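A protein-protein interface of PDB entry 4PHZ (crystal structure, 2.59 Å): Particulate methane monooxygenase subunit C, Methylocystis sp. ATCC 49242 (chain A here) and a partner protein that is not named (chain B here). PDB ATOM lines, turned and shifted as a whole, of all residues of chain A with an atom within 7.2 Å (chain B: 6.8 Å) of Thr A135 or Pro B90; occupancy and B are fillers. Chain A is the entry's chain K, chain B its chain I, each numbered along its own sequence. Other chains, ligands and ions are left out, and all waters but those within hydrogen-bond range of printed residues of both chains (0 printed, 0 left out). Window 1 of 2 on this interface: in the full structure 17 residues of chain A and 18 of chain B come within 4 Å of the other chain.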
ATOM      1  N   GLY A  46      13.258  14.977 -18.781  1.00  0.00           N
ATOM      2  CA  GLY A  46      12.046  14.342 -18.256  1.00  0.00           C
ATOM      3  C   GLY A  46      12.169  12.850 -18.483  1.00  0.00           C
ATOM      4  O   GLY A  46      12.263  12.076 -17.523  1.00  0.00           O
ATOM      5  N   TRP A  47      12.189  12.467 -19.762  1.00  0.00           N
ATOM      6  CA  TRP A  47      12.473  11.096 -20.175  1.00  0.00           C
ATOM      7  C   TRP A  47      13.917  10.755 -20.075  1.00  0.00           C
ATOM      8  O   TRP A  47      14.762  11.345 -20.765  1.00  0.00           O
ATOM      9  CB  TRP A  47      11.994  10.841 -21.589  1.00  0.00           C
ATOM     10  CG  TRP A  47      10.557  10.462 -21.555  1.00  0.00           C
ATOM     11  CD1 TRP A  47      10.006   9.206 -21.290  1.00  0.00           C
ATOM     12  CD2 TRP A  47       9.424  11.345 -21.729  1.00  0.00           C
ATOM     13  NE1 TRP A  47       8.638   9.253 -21.316  1.00  0.00           N
ATOM     14  CE2 TRP A  47       8.220  10.506 -21.574  1.00  0.00           C
ATOM     15  CE3 TRP A  47       9.282  12.692 -22.002  1.00  0.00           C
ATOM     16  CZ2 TRP A  47       6.950  11.023 -21.691  1.00  0.00           C
ATOM     17  CZ3 TRP A  47       7.997  13.200 -22.109  1.00  0.00           C
ATOM     18  CH2 TRP A  47       6.861  12.385 -21.949  1.00  0.00           C
ATOM     19  N   GLY A  50      14.234  11.753 -15.121  1.00  0.00           N
ATOM     20  CA  GLY A  50      13.164  12.055 -14.185  1.00  0.00           C
ATOM     21  C   GLY A  50      12.112  10.988 -13.984  1.00  0.00           C
ATOM     22  O   GLY A  50      10.958  11.317 -13.679  1.00  0.00           O
ATOM     23  N   LEU A  51      12.497   9.716 -14.137  1.00  0.00           N
ATOM     24  CA  LEU A  51      11.565   8.589 -13.968  1.00  0.00           C
ATOM     25  C   LEU A  51      11.871   7.778 -12.717  1.00  0.00           C
ATOM     26  O   LEU A  51      10.958   7.281 -12.054  1.00  0.00           O
ATOM     27  CB  LEU A  51      11.548   7.705 -15.205  1.00  0.00           C
ATOM     28  CG  LEU A  51      11.128   8.375 -16.518  1.00  0.00           C
ATOM     29  CD1 LEU A  51      11.721   7.658 -17.728  1.00  0.00           C
ATOM     30  CD2 LEU A  51       9.613   8.502 -16.632  1.00  0.00           C
ATOM     31  N   GLY A 130      -0.931  16.938 -14.624  1.00  0.00           N
ATOM     32  CA  GLY A 130      -2.012  15.986 -14.874  1.00  0.00           C
ATOM     33  C   GLY A 130      -1.571  14.824 -15.743  1.00  0.00           C
ATOM     34  O   GLY A 130      -1.956  13.675 -15.488  1.00  0.00           O
ATOM     35  N   THR A 131      -0.746  15.137 -16.752  1.00  0.00           N
ATOM     36  CA  THR A 131      -0.236  14.154 -17.719  1.00  0.00           C
ATOM     37  C   THR A 131       1.001  13.395 -17.231  1.00  0.00           C
ATOM     38  O   THR A 131       1.163  12.227 -17.529  1.00  0.00           O
ATOM     39  CB  THR A 131       0.016  14.776 -19.112  1.00  0.00           C
ATOM     40  OG1 THR A 131       0.053  13.731 -20.079  1.00  0.00           O
ATOM     41  CG2 THR A 131       1.335  15.571 -19.192  1.00  0.00           C
ATOM     42  N   TRP A 132       1.867  14.050 -16.478  1.00  0.00           N
ATOM     43  CA  TRP A 132       2.954  13.343 -15.815  1.00  0.00           C
ATOM     44  C   TRP A 132       2.511  12.320 -14.776  1.00  0.00           C
ATOM     45  O   TRP A 132       3.253  11.398 -14.464  1.00  0.00           O
ATOM     46  CB  TRP A 132       3.887  14.338 -15.168  1.00  0.00           C
ATOM     47  CG  TRP A 132       5.196  13.729 -14.763  1.00  0.00           C
ATOM     48  CD1 TRP A 132       5.667  13.489 -13.472  1.00  0.00           C
ATOM     49  CD2 TRP A 132       6.259  13.283 -15.651  1.00  0.00           C
ATOM     50  NE1 TRP A 132       6.925  12.934 -13.507  1.00  0.00           N
ATOM     51  CE2 TRP A 132       7.335  12.778 -14.784  1.00  0.00           C
ATOM     52  CE3 TRP A 132       6.427  13.246 -17.038  1.00  0.00           C
ATOM     53  CZ2 TRP A 132       8.511  12.260 -15.301  1.00  0.00           C
ATOM     54  CZ3 TRP A 132       7.621  12.719 -17.555  1.00  0.00           C
ATOM     55  CH2 TRP A 132       8.637  12.240 -16.709  1.00  0.00           C
ATOM     56  N   HIS A 133       1.317  12.474 -14.212  1.00  0.00           N
ATOM     57  CA  HIS A 133       0.806  11.500 -13.249  1.00  0.00           C
ATOM     58  C   HIS A 133       0.447  10.209 -13.941  1.00  0.00           C
ATOM     59  O   HIS A 133       0.430   9.136 -13.315  1.00  0.00           O
ATOM     60  CB  HIS A 133      -0.401  12.059 -12.487  1.00  0.00           C
ATOM     61  CG  HIS A 133      -0.028  12.945 -11.314  1.00  0.00           C
ATOM     62  ND1 HIS A 133       0.644  12.480 -10.230  1.00  0.00           N
ATOM     63  CD2 HIS A 133      -0.257  14.308 -11.080  1.00  0.00           C
ATOM     64  CE1 HIS A 133       0.841  13.493  -9.355  1.00  0.00           C
ATOM     65  NE2 HIS A 133       0.287  14.611  -9.877  1.00  0.00           N
ATOM     66  N   MET A 134       0.154  10.309 -15.240  1.00  0.00           N
ATOM     67  CA  MET A 134      -0.196   9.158 -16.070  1.00  0.00           C
ATOM     68  C   MET A 134       1.038   8.512 -16.706  1.00  0.00           C
ATOM     69  O   MET A 134       0.934   7.640 -17.567  1.00  0.00           O
ATOM     70  CB  MET A 134      -1.195   9.573 -17.148  1.00  0.00           C
ATOM     71  CG  MET A 134      -2.498  10.099 -16.573  1.00  0.00           C
ATOM     72  SD  MET A 134      -3.279   8.895 -15.489  1.00  0.00           S
ATOM     73  CE  MET A 134      -3.441   9.823 -13.966  1.00  0.00           C
ATOM     74  N   THR A 135       2.203   8.917 -16.224  1.00  0.00           N
ATOM     75  CA  THR A 135       3.490   8.546 -16.790  1.00  0.00           C
ATOM     76  C   THR A 135       4.411   8.036 -15.676  1.00  0.00           C
ATOM     77  O   THR A 135       5.501   7.550 -15.941  1.00  0.00           O
ATOM     78  CB  THR A 135       4.107   9.766 -17.540  1.00  0.00           C
ATOM     79  OG1 THR A 135       3.365  10.021 -18.748  1.00  0.00           O
ATOM     80  CG2 THR A 135       5.587   9.566 -17.875  1.00  0.00           C
ATOM     81  N   VAL A 136       3.975   8.152 -14.428  1.00  0.00           N
ATOM     82  CA  VAL A 136       4.716   7.582 -13.300  1.00  0.00           C
ATOM     83  C   VAL A 136       3.785   7.047 -12.224  1.00  0.00           C
ATOM     84  O   VAL A 136       2.582   7.271 -12.249  1.00  0.00           O
ATOM     85  CB  VAL A 136       5.717   8.569 -12.635  1.00  0.00           C
ATOM     86  CG1 VAL A 136       6.930   8.838 -13.527  1.00  0.00           C
ATOM     87  CG2 VAL A 136       5.019   9.847 -12.202  1.00  0.00           C
ATOM     88  N   ILE A 137       4.374   6.333 -11.276  1.00  0.00           N
ATOM     89  CA  ILE A 137       3.691   5.919 -10.057  1.00  0.00           C
ATOM     90  C   ILE A 137       4.323   6.603  -8.824  1.00  0.00           C
ATOM     91  O   ILE A 137       3.883   6.392  -7.691  1.00  0.00           O
ATOM     92  CB  ILE A 137       3.665   4.384  -9.934  1.00  0.00           C
ATOM     93  CG1 ILE A 137       2.813   3.774 -11.057  1.00  0.00           C
ATOM     94  CG2 ILE A 137       3.136   3.962  -8.578  1.00  0.00           C
ATOM     95  CD1 ILE A 137       3.603   3.348 -12.284  1.00  0.00           C
ATOM     96  N   ARG A 138       5.350   7.423  -9.073  1.00  0.00           N
ATOM     97  CA  ARG A 138       5.913   8.402  -8.114  1.00  0.00           C
ATOM     98  C   ARG A 138       6.761   7.816  -6.959  1.00  0.00           C
ATOM     99  O   ARG A 138       6.243   7.103  -6.095  1.00  0.00           O
ATOM    100  CB  ARG A 138       4.814   9.327  -7.566  1.00  0.00           C
ATOM    101  CG  ARG A 138       3.842   9.873  -8.603  1.00  0.00           C
ATOM    102  CD  ARG A 138       2.718  10.664  -7.952  1.00  0.00           C
ATOM    103  NE  ARG A 138       3.203  11.939  -7.432  1.00  0.00           N
ATOM    104  CZ  ARG A 138       3.706  12.123  -6.211  1.00  0.00           C
ATOM    105  NH1 ARG A 138       4.128  13.325  -5.852  1.00  0.00           N
ATOM    106  NH2 ARG A 138       3.796  11.118  -5.344  1.00  0.00           N
ATOM    107  N   HIS B  29       8.431   2.407 -11.788  1.00  0.00           N
ATOM    108  CA  HIS B  29       9.764   2.476 -11.135  1.00  0.00           C
ATOM    109  C   HIS B  29       9.662   2.819  -9.672  1.00  0.00           C
ATOM    110  O   HIS B  29      10.652   2.694  -8.914  1.00  0.00           O
ATOM    111  CB  HIS B  29      10.638   3.496 -11.850  1.00  0.00           C
ATOM    112  CG  HIS B  29      11.789   2.887 -12.616  1.00  0.00           C
ATOM    113  ND1 HIS B  29      11.897   2.973 -13.958  1.00  0.00           N
ATOM    114  CD2 HIS B  29      12.912   2.174 -12.172  1.00  0.00           C
ATOM    115  CE1 HIS B  29      13.022   2.346 -14.358  1.00  0.00           C
ATOM    116  NE2 HIS B  29      13.641   1.855 -13.261  1.00  0.00           N
ATOM    117  N   ALA B  87      -0.122  -2.484 -17.750  1.00  0.00           N
ATOM    118  CA  ALA B  87       1.303  -2.354 -18.081  1.00  0.00           C
ATOM    119  C   ALA B  87       1.958  -1.154 -17.369  1.00  0.00           C
ATOM    120  O   ALA B  87       1.780   0.007 -17.761  1.00  0.00           O
ATOM    121  CB  ALA B  87       1.474  -2.208 -19.573  1.00  0.00           C
ATOM    122  N   GLY B  88       2.709  -1.442 -16.304  1.00  0.00           N
ATOM    123  CA  GLY B  88       3.542  -0.434 -15.646  1.00  0.00           C
ATOM    124  C   GLY B  88       4.571   0.059 -16.641  1.00  0.00           C
ATOM    125  O   GLY B  88       5.567  -0.605 -16.861  1.00  0.00           O
ATOM    126  N   GLU B  89       4.302   1.215 -17.251  1.00  0.00           N
ATOM    127  CA  GLU B  89       5.136   1.767 -18.316  1.00  0.00           C
ATOM    128  C   GLU B  89       4.985   3.318 -18.506  1.00  0.00           C
ATOM    129  O   GLU B  89       3.852   3.843 -18.518  1.00  0.00           O
ATOM    130  CB  GLU B  89       4.815   0.982 -19.574  1.00  0.00           C
ATOM    131  CG  GLU B  89       4.802   1.724 -20.874  1.00  0.00           C
ATOM    132  CD  GLU B  89       3.661   1.264 -21.765  1.00  0.00           C
ATOM    133  OE1 GLU B  89       2.575   1.021 -21.258  1.00  0.00           O
ATOM    134  OE2 GLU B  89       3.818   1.135 -22.985  1.00  0.00           O
ATOM    135  N   PRO B  90       6.129   4.048 -18.663  1.00  0.00           N
ATOM    136  CA  PRO B  90       6.174   5.532 -18.841  1.00  0.00           C
ATOM    137  C   PRO B  90       5.403   6.073 -20.067  1.00  0.00           C
ATOM    138  O   PRO B  90       6.016   6.568 -21.040  1.00  0.00           O
ATOM    139  CB  PRO B  90       7.681   5.834 -18.982  1.00  0.00           C
ATOM    140  CG  PRO B  90       8.304   4.543 -19.420  1.00  0.00           C
ATOM    141  CD  PRO B  90       7.487   3.453 -18.764  1.00  0.00           C
ATOM    142  N   GLY B  91       4.067   5.992 -20.009  1.00  0.00           N
ATOM    143  CA  GLY B  91       3.187   6.507 -21.079  1.00  0.00           C
ATOM    144  C   GLY B  91       3.168   5.491 -22.193  1.00  0.00           C
ATOM    145  O   GLY B  91       3.850   4.454 -22.094  1.00  0.00           O
ATOM    146  N   PRO B  92       2.411   5.765 -23.271  1.00  0.00           N
ATOM    147  CA  PRO B  92       2.270   4.751 -24.328  1.00  0.00           C
ATOM    148  C   PRO B  92       3.498   4.558 -25.243  1.00  0.00           C
ATOM    149  O   PRO B  92       3.417   4.830 -26.470  1.00  0.00           O
ATOM    150  CB  PRO B  92       1.033   5.207 -25.131  1.00  0.00           C
ATOM    151  CG  PRO B  92       0.677   6.558 -24.615  1.00  0.00           C
ATOM    152  CD  PRO B  92       1.655   6.988 -23.557  1.00  0.00           C
ATOM    153  N   VAL B  93       4.604   4.075 -24.660  1.00  0.00           N
ATOM    154  CA  VAL B  93       5.792   3.716 -25.444  1.00  0.00           C
ATOM    155  C   VAL B  93       5.500   2.413 -26.195  1.00  0.00           C
ATOM    156  O   VAL B  93       6.044   2.162 -27.297  1.00  0.00           O
ATOM    157  CB  VAL B  93       7.112   3.632 -24.619  1.00  0.00           C
ATOM    158  CG1 VAL B  93       7.634   5.023 -24.298  1.00  0.00           C
ATOM    159  CG2 VAL B  93       6.958   2.831 -23.333  1.00  0.00           C
ATOM    160  N   ARG B 128       7.320   3.727 -29.330  1.00  0.00           N
ATOM    161  CA  ARG B 128       8.285   4.812 -29.234  1.00  0.00           C
ATOM    162  C   ARG B 128       9.662   4.304 -28.962  1.00  0.00           C
ATOM    163  O   ARG B 128       9.920   3.702 -27.900  1.00  0.00           O
ATOM    164  CB  ARG B 128       7.914   5.772 -28.123  1.00  0.00           C
ATOM    165  CG  ARG B 128       7.391   7.111 -28.585  1.00  0.00           C
ATOM    166  CD  ARG B 128       7.062   7.945 -27.366  1.00  0.00           C
ATOM    167  NE  ARG B 128       8.250   8.536 -26.754  1.00  0.00           N
ATOM    168  CZ  ARG B 128       8.363   8.853 -25.461  1.00  0.00           C
ATOM    169  NH1 ARG B 128       9.494   9.410 -25.033  1.00  0.00           N
ATOM    170  NH2 ARG B 128       7.357   8.630 -24.597  1.00  0.00           N
ATOM    171  N   TRP B 132      12.932   1.351 -22.482  1.00  0.00           N
ATOM    172  CA  TRP B 132      11.923   1.487 -21.441  1.00  0.00           C
ATOM    173  C   TRP B 132      11.879   0.334 -20.494  1.00  0.00           C
ATOM    174  O   TRP B 132      12.172  -0.780 -20.891  1.00  0.00           O
ATOM    175  CB  TRP B 132      10.597   1.584 -22.136  1.00  0.00           C
ATOM    176  CG  TRP B 132      10.683   2.484 -23.340  1.00  0.00           C
ATOM    177  CD1 TRP B 132      10.547   2.129 -24.675  1.00  0.00           C
ATOM    178  CD2 TRP B 132      10.941   3.925 -23.352  1.00  0.00           C
ATOM    179  NE1 TRP B 132      10.671   3.225 -25.492  1.00  0.00           N
ATOM    180  CE2 TRP B 132      10.907   4.336 -24.761  1.00  0.00           C
ATOM    181  CE3 TRP B 132      11.160   4.885 -22.377  1.00  0.00           C
ATOM    182  CZ2 TRP B 132      11.095   5.663 -25.147  1.00  0.00           C
ATOM    183  CZ3 TRP B 132      11.352   6.214 -22.775  1.00  0.00           C
ATOM    184  CH2 TRP B 132      11.321   6.594 -24.128  1.00  0.00           C
ATOM    185  N   HIS B 133      11.504   0.588 -19.240  1.00  0.00           N
ATOM    186  CA  HIS B 133      11.388  -0.450 -18.211  1.00  0.00           C
ATOM    187  C   HIS B 133       9.933  -0.742 -17.922  1.00  0.00           C
ATOM    188  O   HIS B 133       9.237   0.071 -17.291  1.00  0.00           O
ATOM    189  CB  HIS B 133      12.086  -0.030 -16.954  1.00  0.00           C
ATOM    190  CG  HIS B 133      12.463  -1.164 -16.071  1.00  0.00           C
ATOM    191  ND1 HIS B 133      12.033  -1.260 -14.811  1.00  0.00           N
ATOM    192  CD2 HIS B 133      13.291  -2.261 -16.291  1.00  0.00           C
ATOM    193  CE1 HIS B 133      12.553  -2.371 -14.237  1.00  0.00           C
ATOM    194  NE2 HIS B 133      13.326  -2.981 -15.145  1.00  0.00           N
ATOM    195  N   VAL B 134       9.482  -1.927 -18.366  1.00  0.00           N
ATOM    196  CA  VAL B 134       8.067  -2.299 -18.452  1.00  0.00           C
ATOM    197  C   VAL B 134       7.648  -3.326 -17.394  1.00  0.00           C
ATOM    198  O   VAL B 134       8.143  -4.434 -17.368  1.00  0.00           O
ATOM    199  CB  VAL B 134       7.728  -2.791 -19.869  1.00  0.00           C
ATOM    200  CG1 VAL B 134       6.262  -3.155 -19.965  1.00  0.00           C
ATOM    201  CG2 VAL B 134       8.092  -1.723 -20.895  1.00  0.00           C
ATOM    202  N   HIS B 135       6.728  -2.922 -16.526  1.00  0.00           N
ATOM    203  CA  HIS B 135       6.263  -3.724 -15.399  1.00  0.00           C
ATOM    204  C   HIS B 135       4.898  -4.337 -15.610  1.00  0.00           C
ATOM    205  O   HIS B 135       4.081  -3.886 -16.454  1.00  0.00           O
ATOM    206  CB  HIS B 135       6.138  -2.847 -14.164  1.00  0.00           C
ATOM    207  CG  HIS B 135       7.436  -2.283 -13.663  1.00  0.00           C
ATOM    208  ND1 HIS B 135       8.029  -2.717 -12.512  1.00  0.00           N
ATOM    209  CD2 HIS B 135       8.245  -1.274 -14.172  1.00  0.00           C
ATOM    210  CE1 HIS B 135       9.168  -2.026 -12.311  1.00  0.00           C
ATOM    211  NE2 HIS B 135       9.296  -1.130 -13.318  1.00  0.00           N
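OG1 of Thr A135 sits at hydrogen-bond distance from O of Thr A131, at 3.3 Å.
NE1 of Trp B132 is in hydrogen-bond range of O of Arg B128 (2.6 Å).
The backbone carbonyl oxygen (O) of Val B93 is in hydrogen-bond range of the backbone NH (N) of Arg B128, 2.9 Å away.
Pro B90 touches Trp A47.
Trp A47 touches Arg B128.
CZ3 of Trp B132 touches CD1 of Trp A47 (3.6 Å).
O of Leu A51 touches CB of His B29, at 3.8 Å.
O of Thr A135 touches CA of Pro B90, at 3.6 Å.
Of chain B, only Pro B90 comes within 4 Å of Thr A135.
Pro B90 touches just these residues of chain A: Trp A47 and Thr A135.
No residue of chain A comes within 4 Å of Gly B91.
Of the printed residues of chain A, Trp B132 touches Trp A47 (3.6 Å).
Printed residues of chain B within 4 Å of Leu A51: His B29.
Printed residues of chain A within 4 Å of Arg B128: Trp A47 (3.6 Å).
Printed residues of chain A within 4 Å of His B29: Leu A51 (3.8 Å).
The nearest printed residue of chain A that does not touch Arg B128 is Thr A135 (7.0 Å).
Of the 13 printed residues of chain A, 3 touch a printed residue of chain B.
Hydrophobic or aromatic side chains of chain A within 4 Å of the printed part of chain B: Trp A47.
Printed residues of chain B that touch a printed residue of chain A: His B29, Pro B90, Arg B128 and Trp B132.
Among the printed residues, 5 pairs touch across the chains.
Among the printed residues, no Asp or Glu carboxylate lies within 4 Å of a Lys or Arg side-chain nitrogen of the other chain.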
